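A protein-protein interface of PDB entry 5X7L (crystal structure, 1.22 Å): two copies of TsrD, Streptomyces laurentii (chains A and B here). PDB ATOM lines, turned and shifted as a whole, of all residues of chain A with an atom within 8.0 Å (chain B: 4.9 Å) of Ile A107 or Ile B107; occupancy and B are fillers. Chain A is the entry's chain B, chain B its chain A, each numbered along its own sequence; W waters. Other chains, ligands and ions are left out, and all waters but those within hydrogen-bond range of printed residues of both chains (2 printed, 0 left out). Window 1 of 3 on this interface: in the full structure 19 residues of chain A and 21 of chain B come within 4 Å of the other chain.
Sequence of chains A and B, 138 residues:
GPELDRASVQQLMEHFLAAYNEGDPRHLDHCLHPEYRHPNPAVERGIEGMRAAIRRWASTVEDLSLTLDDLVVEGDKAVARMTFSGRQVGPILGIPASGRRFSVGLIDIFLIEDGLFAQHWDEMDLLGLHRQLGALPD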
ATOM      1  N   ASP A  69       4.252 -10.068  20.835  1.00  0.00           N
ATOM      2  CA  ASP A  69       4.146 -10.374  22.260  1.00  0.00           C
ATOM      3  C   ASP A  69       3.326 -11.627  22.521  1.00  0.00           C
ATOM      4  O   ASP A  69       3.605 -12.370  23.459  1.00  0.00           O
ATOM      5  CB  ASP A  69       3.522  -9.198  23.007  1.00  0.00           C
ATOM      6  CG  ASP A  69       4.366  -7.949  22.926  1.00  0.00           C
ATOM      7  OD1 ASP A  69       5.554  -8.010  23.301  1.00  0.00           O
ATOM      8  OD2 ASP A  69       3.840  -6.906  22.483  1.00  0.00           O
ATOM      9  N   ASP A  70       2.293 -11.843  21.715  1.00  0.00           N
ATOM     10  CA  ASP A  70       1.451 -13.023  21.864  1.00  0.00           C
ATOM     11  C   ASP A  70       0.708 -13.277  20.562  1.00  0.00           C
ATOM     12  O   ASP A  70       0.452 -12.351  19.790  1.00  0.00           O
ATOM     13  CB  ASP A  70       0.463 -12.841  23.028  1.00  0.00           C
ATOM     14  CG  ASP A  70      -0.102 -14.159  23.545  1.00  0.00           C
ATOM     15  OD1 ASP A  70       0.369 -15.239  23.128  1.00  0.00           O
ATOM     16  OD2 ASP A  70      -1.024 -14.116  24.386  1.00  0.00           O
ATOM     17  N   ALA A  78      -6.607 -15.093  13.490  1.00  0.00           N
ATOM     18  CA  ALA A  78      -5.311 -14.975  14.144  1.00  0.00           C
ATOM     19  C   ALA A  78      -5.258 -13.648  14.881  1.00  0.00           C
ATOM     20  O   ALA A  78      -5.536 -12.603  14.299  1.00  0.00           O
ATOM     21  CB  ALA A  78      -4.187 -15.060  13.126  1.00  0.00           C
ATOM     22  N   VAL A  79      -4.912 -13.698  16.162  1.00  0.00           N
ATOM     23  CA  VAL A  79      -4.798 -12.496  16.977  1.00  0.00           C
ATOM     24  C   VAL A  79      -3.344 -12.281  17.355  1.00  0.00           C
ATOM     25  O   VAL A  79      -2.733 -13.143  17.983  1.00  0.00           O
ATOM     26  CB  VAL A  79      -5.638 -12.593  18.260  1.00  0.00           C
ATOM     27  CG1 VAL A  79      -5.535 -11.295  19.051  1.00  0.00           C
ATOM     28  CG2 VAL A  79      -7.085 -12.919  17.919  1.00  0.00           C
ATOM     29  N   ALA A  80      -2.796 -11.135  16.960  1.00  0.00           N
ATOM     30  CA  ALA A  80      -1.411 -10.791  17.256  1.00  0.00           C
ATOM     31  C   ALA A  80      -1.360  -9.575  18.173  1.00  0.00           C
ATOM     32  O   ALA A  80      -1.816  -8.493  17.800  1.00  0.00           O
ATOM     33  CB  ALA A  80      -0.648 -10.516  15.967  1.00  0.00           C
ATOM     34  N   ARG A  81      -0.827  -9.765  19.378  1.00  0.00           N
ATOM     35  CA  ARG A  81      -0.526  -8.647  20.260  1.00  0.00           C
ATOM     36  C   ARG A  81       0.925  -8.262  20.020  1.00  0.00           C
ATOM     37  O   ARG A  81       1.814  -9.115  20.095  1.00  0.00           O
ATOM     38  CB  ARG A  81      -0.749  -9.014  21.728  1.00  0.00           C
ATOM     39  CG  ARG A  81      -0.447  -7.862  22.676  1.00  0.00           C
ATOM     40  CD  ARG A  81      -0.982  -8.084  24.074  1.00  0.00           C
ATOM     41  NE  ARG A  81      -0.344  -9.199  24.769  1.00  0.00           N
ATOM     42  CZ  ARG A  81       0.803  -9.120  25.443  1.00  0.00           C
ATOM     43  NH1 ARG A  81       1.478  -7.975  25.503  1.00  0.00           N
ATOM     44  NH2 ARG A  81       1.283 -10.195  26.060  1.00  0.00           N
ATOM     45  N   MET A  82       1.165  -6.986  19.728  1.00  0.00           N
ATOM     46  CA  MET A  82       2.478  -6.527  19.287  1.00  0.00           C
ATOM     47  C   MET A  82       2.888  -5.248  19.981  1.00  0.00           C
ATOM     48  O   MET A  82       2.060  -4.545  20.572  1.00  0.00           O
ATOM     49  CB  MET A  82       2.473  -6.319  17.768  1.00  0.00           C
ATOM     50  CG  MET A  82       2.300  -7.632  17.012  1.00  0.00           C
ATOM     51  SD  MET A  82       2.050  -7.391  15.092  1.00  0.00           S
ATOM     52  CE  MET A  82       0.180  -6.854  15.142  1.00  0.00           C
ATOM     53  N   THR A  83       4.186  -4.963  19.908  1.00  0.00           N
ATOM     54  CA  THR A  83       4.765  -3.716  20.385  1.00  0.00           C
ATOM     55  C   THR A  83       5.435  -3.024  19.200  1.00  0.00           C
ATOM     56  O   THR A  83       6.201  -3.645  18.462  1.00  0.00           O
ATOM     57  CB  THR A  83       5.785  -3.961  21.511  1.00  0.00           C
ATOM     58  OG1 THR A  83       5.115  -4.542  22.634  1.00  0.00           O
ATOM     59  CG2 THR A  83       6.433  -2.656  21.951  1.00  0.00           C
ATOM     60  N   VAL A 104       4.505   1.746  21.656  1.00  0.00           N
ATOM     61  CA  VAL A 104       3.094   1.536  21.970  1.00  0.00           C
ATOM     62  C   VAL A 104       2.657   0.120  21.645  1.00  0.00           C
ATOM     63  O   VAL A 104       3.222  -0.545  20.776  1.00  0.00           O
ATOM     64  CB  VAL A 104       2.171   2.526  21.217  1.00  0.00           C
ATOM     65  CG1 VAL A 104       2.408   3.944  21.706  1.00  0.00           C
ATOM     66  CG2 VAL A 104       2.365   2.426  19.709  1.00  0.00           C
ATOM     67  N   GLY A 105       1.623  -0.325  22.346  1.00  0.00           N
ATOM     68  CA  GLY A 105       1.045  -1.628  22.098  1.00  0.00           C
ATOM     69  C   GLY A 105      -0.092  -1.564  21.099  1.00  0.00           C
ATOM     70  O   GLY A 105      -0.748  -0.529  20.922  1.00  0.00           O
ATOM     71  N   LEU A 106      -0.323  -2.690  20.436  1.00  0.00           N
ATOM     72  CA  LEU A 106      -1.464  -2.841  19.548  1.00  0.00           C
ATOM     73  C   LEU A 106      -1.892  -4.297  19.559  1.00  0.00           C
ATOM     74  O   LEU A 106      -1.110  -5.185  19.918  1.00  0.00           O
ATOM     75  CB  LEU A 106      -1.118  -2.378  18.126  1.00  0.00           C
ATOM     76  CG  LEU A 106       0.001  -3.152  17.412  1.00  0.00           C
ATOM     77  CD1 LEU A 106      -0.251  -3.256  15.912  1.00  0.00           C
ATOM     78  CD2 LEU A 106       1.383  -2.579  17.693  1.00  0.00           C
ATOM     79  N   ILE A 107      -3.146  -4.527  19.191  1.00  0.00           N
ATOM     80  CA  ILE A 107      -3.649  -5.873  18.970  1.00  0.00           C
ATOM     81  C   ILE A 107      -4.376  -5.881  17.632  1.00  0.00           C
ATOM     82  O   ILE A 107      -5.283  -5.077  17.413  1.00  0.00           O
ATOM     83  CB  ILE A 107      -4.597  -6.342  20.091  1.00  0.00           C
ATOM     84  CG1 ILE A 107      -3.888  -6.297  21.449  1.00  0.00           C
ATOM     85  CG2 ILE A 107      -5.109  -7.745  19.784  1.00  0.00           C
ATOM     86  CD1 ILE A 107      -4.801  -6.537  22.636  1.00  0.00           C
ATOM     87  N   ASP A 108      -3.957  -6.781  16.742  1.00  0.00           N
ATOM     88  CA  ASP A 108      -4.612  -6.995  15.451  1.00  0.00           C
ATOM     89  C   ASP A 108      -5.306  -8.346  15.444  1.00  0.00           C
ATOM     90  O   ASP A 108      -4.711  -9.351  15.836  1.00  0.00           O
ATOM     91  CB  ASP A 108      -3.598  -6.997  14.300  1.00  0.00           C
ATOM     92  CG  ASP A 108      -3.009  -5.632  14.011  1.00  0.00           C
ATOM     93  OD1 ASP A 108      -3.404  -4.631  14.641  1.00  0.00           O
ATOM     94  OD2 ASP A 108      -2.131  -5.568  13.129  1.00  0.00           O
ATOM     95  N   ILE A 109      -6.552  -8.363  14.981  1.00  0.00           N
ATOM     96  CA  ILE A 109      -7.260  -9.603  14.702  1.00  0.00           C
ATOM     97  C   ILE A 109      -7.370  -9.730  13.192  1.00  0.00           C
ATOM     98  O   ILE A 109      -7.948  -8.864  12.542  1.00  0.00           O
ATOM     99  CB  ILE A 109      -8.662  -9.623  15.334  1.00  0.00           C
ATOM    100  CG1 ILE A 109      -8.560  -9.432  16.849  1.00  0.00           C
ATOM    101  CG2 ILE A 109      -9.378 -10.924  14.987  1.00  0.00           C
ATOM    102  CD1 ILE A 109      -9.892  -9.301  17.549  1.00  0.00           C
ATOM    103  N   PHE A 110      -6.807 -10.802  12.641  1.00  0.00           N
ATOM    104  CA  PHE A 110      -6.844 -11.055  11.205  1.00  0.00           C
ATOM    105  C   PHE A 110      -7.834 -12.156  10.860  1.00  0.00           C
ATOM    106  O   PHE A 110      -7.917 -13.170  11.554  1.00  0.00           O
ATOM    107  CB  PHE A 110      -5.474 -11.489  10.690  1.00  0.00           C
ATOM    108  CG  PHE A 110      -4.404 -10.448  10.815  1.00  0.00           C
ATOM    109  CD1 PHE A 110      -4.343  -9.384   9.925  1.00  0.00           C
ATOM    110  CD2 PHE A 110      -3.432 -10.551  11.799  1.00  0.00           C
ATOM    111  CE1 PHE A 110      -3.341  -8.432  10.026  1.00  0.00           C
ATOM    112  CE2 PHE A 110      -2.430  -9.598  11.906  1.00  0.00           C
ATOM    113  CZ  PHE A 110      -2.383  -8.541  11.016  1.00  0.00           C
ATOM    114  N   HIS A 120      -8.619  -7.077   8.695  1.00  0.00           N
ATOM    115  CA  HIS A 120      -8.283  -6.979  10.115  1.00  0.00           C
ATOM    116  C   HIS A 120      -9.204  -6.038  10.870  1.00  0.00           C
ATOM    117  O   HIS A 120      -9.868  -5.183  10.283  1.00  0.00           O
ATOM    118  CB  HIS A 120      -6.829  -6.535  10.324  1.00  0.00           C
ATOM    119  CG  HIS A 120      -6.575  -5.098   9.985  1.00  0.00           C
ATOM    120  ND1 HIS A 120      -6.082  -4.703   8.761  1.00  0.00           N
ATOM    121  CD2 HIS A 120      -6.747  -3.966  10.707  1.00  0.00           C
ATOM    122  CE1 HIS A 120      -5.960  -3.388   8.743  1.00  0.00           C
ATOM    123  NE2 HIS A 120      -6.361  -2.916   9.909  1.00  0.00           N
ATOM    124  N   TRP A 121      -9.214  -6.229  12.186  1.00  0.00           N
ATOM    125  CA  TRP A 121      -9.804  -5.318  13.156  1.00  0.00           C
ATOM    126  C   TRP A 121      -8.715  -5.097  14.188  1.00  0.00           C
ATOM    127  O   TRP A 121      -8.063  -6.052  14.603  1.00  0.00           O
ATOM    128  CB  TRP A 121     -11.025  -5.927  13.841  1.00  0.00           C
ATOM    129  CG  TRP A 121     -12.103  -6.397  12.922  1.00  0.00           C
ATOM    130  CD1 TRP A 121     -13.237  -5.720  12.577  1.00  0.00           C
ATOM    131  CD2 TRP A 121     -12.162  -7.657  12.238  1.00  0.00           C
ATOM    132  NE1 TRP A 121     -13.998  -6.479  11.720  1.00  0.00           N
ATOM    133  CE2 TRP A 121     -13.362  -7.672  11.497  1.00  0.00           C
ATOM    134  CE3 TRP A 121     -11.318  -8.776  12.184  1.00  0.00           C
ATOM    135  CZ2 TRP A 121     -13.741  -8.759  10.710  1.00  0.00           C
ATOM    136  CZ3 TRP A 121     -11.696  -9.855  11.400  1.00  0.00           C
ATOM    137  CH2 TRP A 121     -12.900  -9.838  10.675  1.00  0.00           C
ATOM    138  N   ASP A 122      -8.506  -3.863  14.622  1.00  0.00           N
ATOM    139  CA  ASP A 122      -7.384  -3.599  15.513  1.00  0.00           C
ATOM    140  C   ASP A 122      -7.693  -2.539  16.552  1.00  0.00           C
ATOM    141  O   ASP A 122      -8.662  -1.787  16.426  1.00  0.00           O
ATOM    142  CB  ASP A 122      -6.162  -3.173  14.701  1.00  0.00           C
ATOM    143  CG  ASP A 122      -6.334  -1.813  14.072  1.00  0.00           C
ATOM    144  OD1 ASP A 122      -7.182  -1.679  13.167  1.00  0.00           O
ATOM    145  OD2 ASP A 122      -5.623  -0.876  14.485  1.00  0.00           O
ATOM    146  N   GLU A 123      -6.862  -2.512  17.590  1.00  0.00           N
ATOM    147  CA  GLU A 123      -6.776  -1.382  18.502  1.00  0.00           C
ATOM    148  C   GLU A 123      -5.303  -1.126  18.799  1.00  0.00           C
ATOM    149  O   GLU A 123      -4.528  -2.063  19.001  1.00  0.00           O
ATOM    150  CB  GLU A 123      -7.527  -1.638  19.809  1.00  0.00           C
ATOM    151  CG  GLU A 123      -9.017  -1.911  19.672  1.00  0.00           C
ATOM    152  CD  GLU A 123      -9.832  -0.728  19.177  1.00  0.00           C
ATOM    153  OE1 GLU A 123      -9.316   0.406  19.095  1.00  0.00           O
ATOM    154  OE2 GLU A 123     -11.017  -0.946  18.866  1.00  0.00           O
ATOM    155  N   MET A 124      -4.924   0.148  18.806  1.00  0.00           N
ATOM    156  CA  MET A 124      -3.565   0.580  19.134  1.00  0.00           C
ATOM    157  C   MET A 124      -3.675   1.659  20.189  1.00  0.00           C
ATOM    158  O   MET A 124      -4.666   2.392  20.224  1.00  0.00           O
ATOM    159  CB  MET A 124      -2.844   1.101  17.879  1.00  0.00           C
ATOM    160  CG  MET A 124      -1.511   1.797  18.174  1.00  0.00           C
ATOM    161  SD  MET A 124      -0.601   2.480  16.574  1.00  0.00           S
ATOM    162  CE  MET A 124       0.208   0.769  16.171  1.00  0.00           C
ATOM    163  N   ASP A 125      -2.664   1.767  21.046  1.00  0.00           N
ATOM    164  CA  ASP A 125      -2.632   2.811  22.072  1.00  0.00           C
ATOM    165  C   ASP A 125      -2.291   4.177  21.457  1.00  0.00           C
ATOM    166  O   ASP A 125      -1.194   4.710  21.655  1.00  0.00           O
ATOM    167  CB  ASP A 125      -1.624   2.430  23.161  1.00  0.00           C
ATOM    168  CG  ASP A 125      -1.585   3.416  24.316  1.00  0.00           C
ATOM    169  OD1 ASP A 125      -2.515   4.242  24.447  1.00  0.00           O
ATOM    170  OD2 ASP A 125      -0.611   3.357  25.096  1.00  0.00           O
ATOM    171  N   VAL B  79      -9.677 -14.182  23.479  1.00  0.00           N
ATOM    172  CA  VAL B  79      -9.610 -12.826  22.945  1.00  0.00           C
ATOM    173  C   VAL B  79     -11.017 -12.334  22.675  1.00  0.00           C
ATOM    174  O   VAL B  79     -11.747 -12.943  21.896  1.00  0.00           O
ATOM    175  CB  VAL B  79      -8.805 -12.760  21.640  1.00  0.00           C
ATOM    176  CG1 VAL B  79      -8.726 -11.318  21.151  1.00  0.00           C
ATOM    177  CG2 VAL B  79      -7.420 -13.356  21.837  1.00  0.00           C
ATOM    178  N   ALA B  80     -11.383 -11.232  23.321  1.00  0.00           N
ATOM    179  CA  ALA B  80     -12.697 -10.635  23.160  1.00  0.00           C
ATOM    180  C   ALA B  80     -12.560  -9.260  22.520  1.00  0.00           C
ATOM    181  O   ALA B  80     -11.984  -8.352  23.117  1.00  0.00           O
ATOM    182  CB  ALA B  80     -13.385 -10.529  24.511  1.00  0.00           C
ATOM    183  N   ARG B  81     -13.086  -9.113  21.306  1.00  0.00           N
ATOM    184  CA  ARG B  81     -13.224  -7.796  20.698  1.00  0.00           C
ATOM    185  C   ARG B  81     -14.595  -7.264  21.085  1.00  0.00           C
ATOM    186  O   ARG B  81     -15.608  -7.931  20.857  1.00  0.00           O
ATOM    187  CB  ARG B  81     -13.080  -7.847  19.177  1.00  0.00           C
ATOM    188  CG  ARG B  81     -13.231  -6.475  18.526  1.00  0.00           C
ATOM    189  CD  ARG B  81     -12.832  -6.453  17.060  1.00  0.00           C
ATOM    190  NE  ARG B  81     -13.802  -7.102  16.170  1.00  0.00           N
ATOM    191  CZ  ARG B  81     -14.936  -6.541  15.737  1.00  0.00           C
ATOM    192  NH1 ARG B  81     -15.278  -5.322  16.139  1.00  0.00           N
ATOM    193  NH2 ARG B  81     -15.744  -7.198  14.908  1.00  0.00           N
ATOM    194  N   GLY B 105     -14.163   1.028  20.694  1.00  0.00           N
ATOM    195  CA  GLY B 105     -13.750  -0.361  20.650  1.00  0.00           C
ATOM    196  C   GLY B 105     -12.647  -0.688  21.635  1.00  0.00           C
ATOM    197  O   GLY B 105     -11.874   0.180  22.059  1.00  0.00           O
ATOM    198  N   LEU B 106     -12.581  -1.960  21.997  1.00  0.00           N
ATOM    199  CA  LEU B 106     -11.472  -2.475  22.778  1.00  0.00           C
ATOM    200  C   LEU B 106     -11.240  -3.926  22.394  1.00  0.00           C
ATOM    201  O   LEU B 106     -12.119  -4.578  21.821  1.00  0.00           O
ATOM    202  CB  LEU B 106     -11.756  -2.340  24.275  1.00  0.00           C
ATOM    203  CG  LEU B 106     -13.014  -3.068  24.768  1.00  0.00           C
ATOM    204  CD1 LEU B 106     -12.742  -3.835  26.052  1.00  0.00           C
ATOM    205  CD2 LEU B 106     -14.224  -2.144  24.872  1.00  0.00           C
ATOM    206  N   ILE B 107     -10.040  -4.414  22.681  1.00  0.00           N
ATOM    207  CA  ILE B 107      -9.747  -5.832  22.569  1.00  0.00           C
ATOM    208  C   ILE B 107      -9.042  -6.251  23.850  1.00  0.00           C
ATOM    209  O   ILE B 107      -8.016  -5.672  24.219  1.00  0.00           O
ATOM    210  CB  ILE B 107      -8.866  -6.172  21.347  1.00  0.00           C
ATOM    211  CG1 ILE B 107      -9.541  -5.732  20.041  1.00  0.00           C
ATOM    212  CG2 ILE B 107      -8.573  -7.668  21.315  1.00  0.00           C
ATOM    213  CD1 ILE B 107      -8.628  -5.771  18.828  1.00  0.00           C
ATOM    214  N   ASP B 108      -9.620  -7.239  24.532  1.00  0.00           N
ATOM    215  CA  ASP B 108      -9.030  -7.835  25.727  1.00  0.00           C
ATOM    216  C   ASP B 108      -8.554  -9.243  25.412  1.00  0.00           C
ATOM    217  O   ASP B 108      -9.287 -10.026  24.800  1.00  0.00           O
ATOM    218  CB  ASP B 108     -10.051  -7.935  26.863  1.00  0.00           C
ATOM    219  CG  ASP B 108     -10.444  -6.599  27.436  1.00  0.00           C
ATOM    220  OD1 ASP B 108      -9.889  -5.561  27.028  1.00  0.00           O
ATOM    221  OD2 ASP B 108     -11.326  -6.596  28.318  1.00  0.00           O
ATOM    222  N   ILE B 109      -7.339  -9.567  25.848  1.00  0.00           N
ATOM    223  CA  ILE B 109      -6.847 -10.939  25.820  1.00  0.00           C
ATOM    224  C   ILE B 109      -6.788 -11.416  27.262  1.00  0.00           C
ATOM    225  O   ILE B 109      -6.054 -10.843  28.070  1.00  0.00           O
ATOM    226  CB  ILE B 109      -5.454 -11.057  25.169  1.00  0.00           C
ATOM    227  CG1 ILE B 109      -5.480 -10.469  23.752  1.00  0.00           C
ATOM    228  CG2 ILE B 109      -4.994 -12.519  25.162  1.00  0.00           C
ATOM    229  CD1 ILE B 109      -4.152 -10.531  23.020  1.00  0.00           C
ATOM    230  N   TRP B 121      -4.426  -8.586  29.014  1.00  0.00           N
ATOM    231  CA  TRP B 121      -3.707  -7.564  28.271  1.00  0.00           C
ATOM    232  C   TRP B 121      -4.745  -6.946  27.345  1.00  0.00           C
ATOM    233  O   TRP B 121      -5.587  -7.659  26.804  1.00  0.00           O
ATOM    234  CB  TRP B 121      -2.582  -8.168  27.435  1.00  0.00           C
ATOM    235  CG  TRP B 121      -1.597  -9.014  28.185  1.00  0.00           C
ATOM    236  CD1 TRP B 121      -0.371  -8.629  28.645  1.00  0.00           C
ATOM    237  CD2 TRP B 121      -1.735 -10.402  28.526  1.00  0.00           C
ATOM    238  NE1 TRP B 121       0.261  -9.687  29.255  1.00  0.00           N
ATOM    239  CE2 TRP B 121      -0.555 -10.787  29.196  1.00  0.00           C
ATOM    240  CE3 TRP B 121      -2.742 -11.354  28.331  1.00  0.00           C
ATOM    241  CZ2 TRP B 121      -0.354 -12.083  29.673  1.00  0.00           C
ATOM    242  CZ3 TRP B 121      -2.540 -12.643  28.803  1.00  0.00           C
ATOM    243  CH2 TRP B 121      -1.354 -12.996  29.465  1.00  0.00           C
ATOM    244  N   ASP B 122      -4.692  -5.642  27.133  1.00  0.00           N
ATOM    245  CA  ASP B 122      -5.727  -5.015  26.330  1.00  0.00           C
ATOM    246  C   ASP B 122      -5.241  -3.785  25.600  1.00  0.00           C
ATOM    247  O   ASP B 122      -4.206  -3.210  25.935  1.00  0.00           O
ATOM    248  CB  ASP B 122      -6.911  -4.622  27.213  1.00  0.00           C
ATOM    249  CG  ASP B 122      -6.579  -3.484  28.152  1.00  0.00           C
ATOM    250  OD1 ASP B 122      -5.688  -3.663  29.007  1.00  0.00           O
ATOM    251  OD2 ASP B 122      -7.196  -2.408  28.021  1.00  0.00           O
ATOM    252  N   GLU B 123      -6.008  -3.396  24.588  1.00  0.00           N
ATOM    253  CA  GLU B 123      -5.926  -2.059  24.028  1.00  0.00           C
ATOM    254  C   GLU B 123      -7.347  -1.561  23.824  1.00  0.00           C
ATOM    255  O   GLU B 123      -8.236  -2.318  23.428  1.00  0.00           O
ATOM    256  CB  GLU B 123      -5.154  -2.029  22.707  1.00  0.00           C
ATOM    257  CG  GLU B 123      -3.725  -2.546  22.788  1.00  0.00           C
ATOM    258  CD  GLU B 123      -2.798  -1.702  23.649  1.00  0.00           C
ATOM    259  OE1 GLU B 123      -3.154  -0.566  24.024  1.00  0.00           O
ATOM    260  OE2 GLU B 123      -1.691  -2.190  23.951  1.00  0.00           O
HETATM  261  O   HOH W   1      -0.828  -4.598  23.009  1.00  0.00           O
HETATM  262  O   HOH W   2     -12.326  -3.281  19.055  1.00  0.00           O
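Of the 11 printed residues of chain B, 8 touch a printed residue of chain A. Printed residues of chain B that touch a printed residue of chain A: Val B79, Arg B81, Gly B105, Leu B106, Ile B107, Ile B109, Trp B121 and Glu B123. Printed residues of chain A that touch a printed residue of chain B: Val A79, Arg A81, Gly A105, Leu A106, Ile A107, Ile A109, Trp A121, Glu A123 and Asp A125. Hydrophobic or aromatic side chains of chain A within 4 Å of the printed part of chain B: Val A79, Ile A107, Ile A109 and Trp A121. Along chain A the printed residues that touch a printed residue of chain B span positions 79 to 125.
The indole nitrogen (NE1) of Trp B121 sits close to the guanidinium group (NH2) of Arg A81, at 3.4 Å. OE2 of Glu A123 sits close to O of Gly B105, at 3.5 Å.
Of chain B, only Ile B107 and Glu B123 come within 4 Å of Ile A107. Ile B107 touches just these residues of chain A: Ile A107, Ile A109 and Glu A123. Printed residues of chain A within 4 Å of Ile B109: Arg A81 (3.9 Å). Of the printed residues of chain B, Glu A123 touches Gly B105, Leu B106, Ile B107 and Glu B123. Of the printed residues of chain A, Glu B123 touches Gly A105, Leu A106, Ile A107, Glu A123 and Asp A125. Printed residues of chain A within 4 Å of Gly B105: Glu A123. Ala A78 touches none of the printed residues of chain B. Met A82 touches none of the printed residues of chain B. The nearest printed residue of chain A that does not touch Leu B106 is Ile A109 (6.7 Å).
Among the printed residues, merely in contact across the chains: Gly A105 with Glu B123, Asp A125 with Glu B123, Glu A123 with Leu B106, Trp A121 with Arg B81, Ile A107 with Ile B107, Glu A123 with Glu B123, Leu A106 with Glu B123, Val A79 with Val B79, Ile A109 with Arg B81, Glu A123 with Ile B107, Ile A107 with Glu B123, Arg A81 with Ile B109 and Ile A109 with Ile B107.
Water W2 bridges the side-chain carboxylate of Glu A123 (2.7 Å) and the backbone carbonyl oxygen of Leu B106 (3.1 Å). Water W1 lies within hydrogen-bond range of the side-chain carboxylate (OE2) of Glu B123 and the backbone carbonyl oxygen (O) of Leu A106.
Val B79 touches its own counterpart, Val A79. Leu A106 touches Glu B123, and with the chains exchanged Glu A123 touches Leu B106. Ile B107 touches its own counterpart, Ile A107. Glu B123 touches its own counterpart, Glu A123. Of the 15 pairs that touch across the chains among the printed residues, 13 have their exchanged pair printed and touching as well.
N of Ile B107 is in hydrogen-bond range of O of Glu B123, 2.9 Å away. The backbone NH of Ile B109 sits at hydrogen-bond distance from the backbone carbonyl oxygen of Trp B121 (2.8 Å). The side-chain carboxylate of Asp A69 lies within salt-bridge range of the guanidinium group of Arg A81. The backbone NH (N) of Arg A81 sits at hydrogen-bond distance from the backbone carbonyl oxygen (O) of Asp A70, at 2.9 Å. O of Gly A105 sits at hydrogen-bond distance from N of Asp A125 (3.0 Å). N of Ile A109 is in hydrogen-bond range of O of Trp A121.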
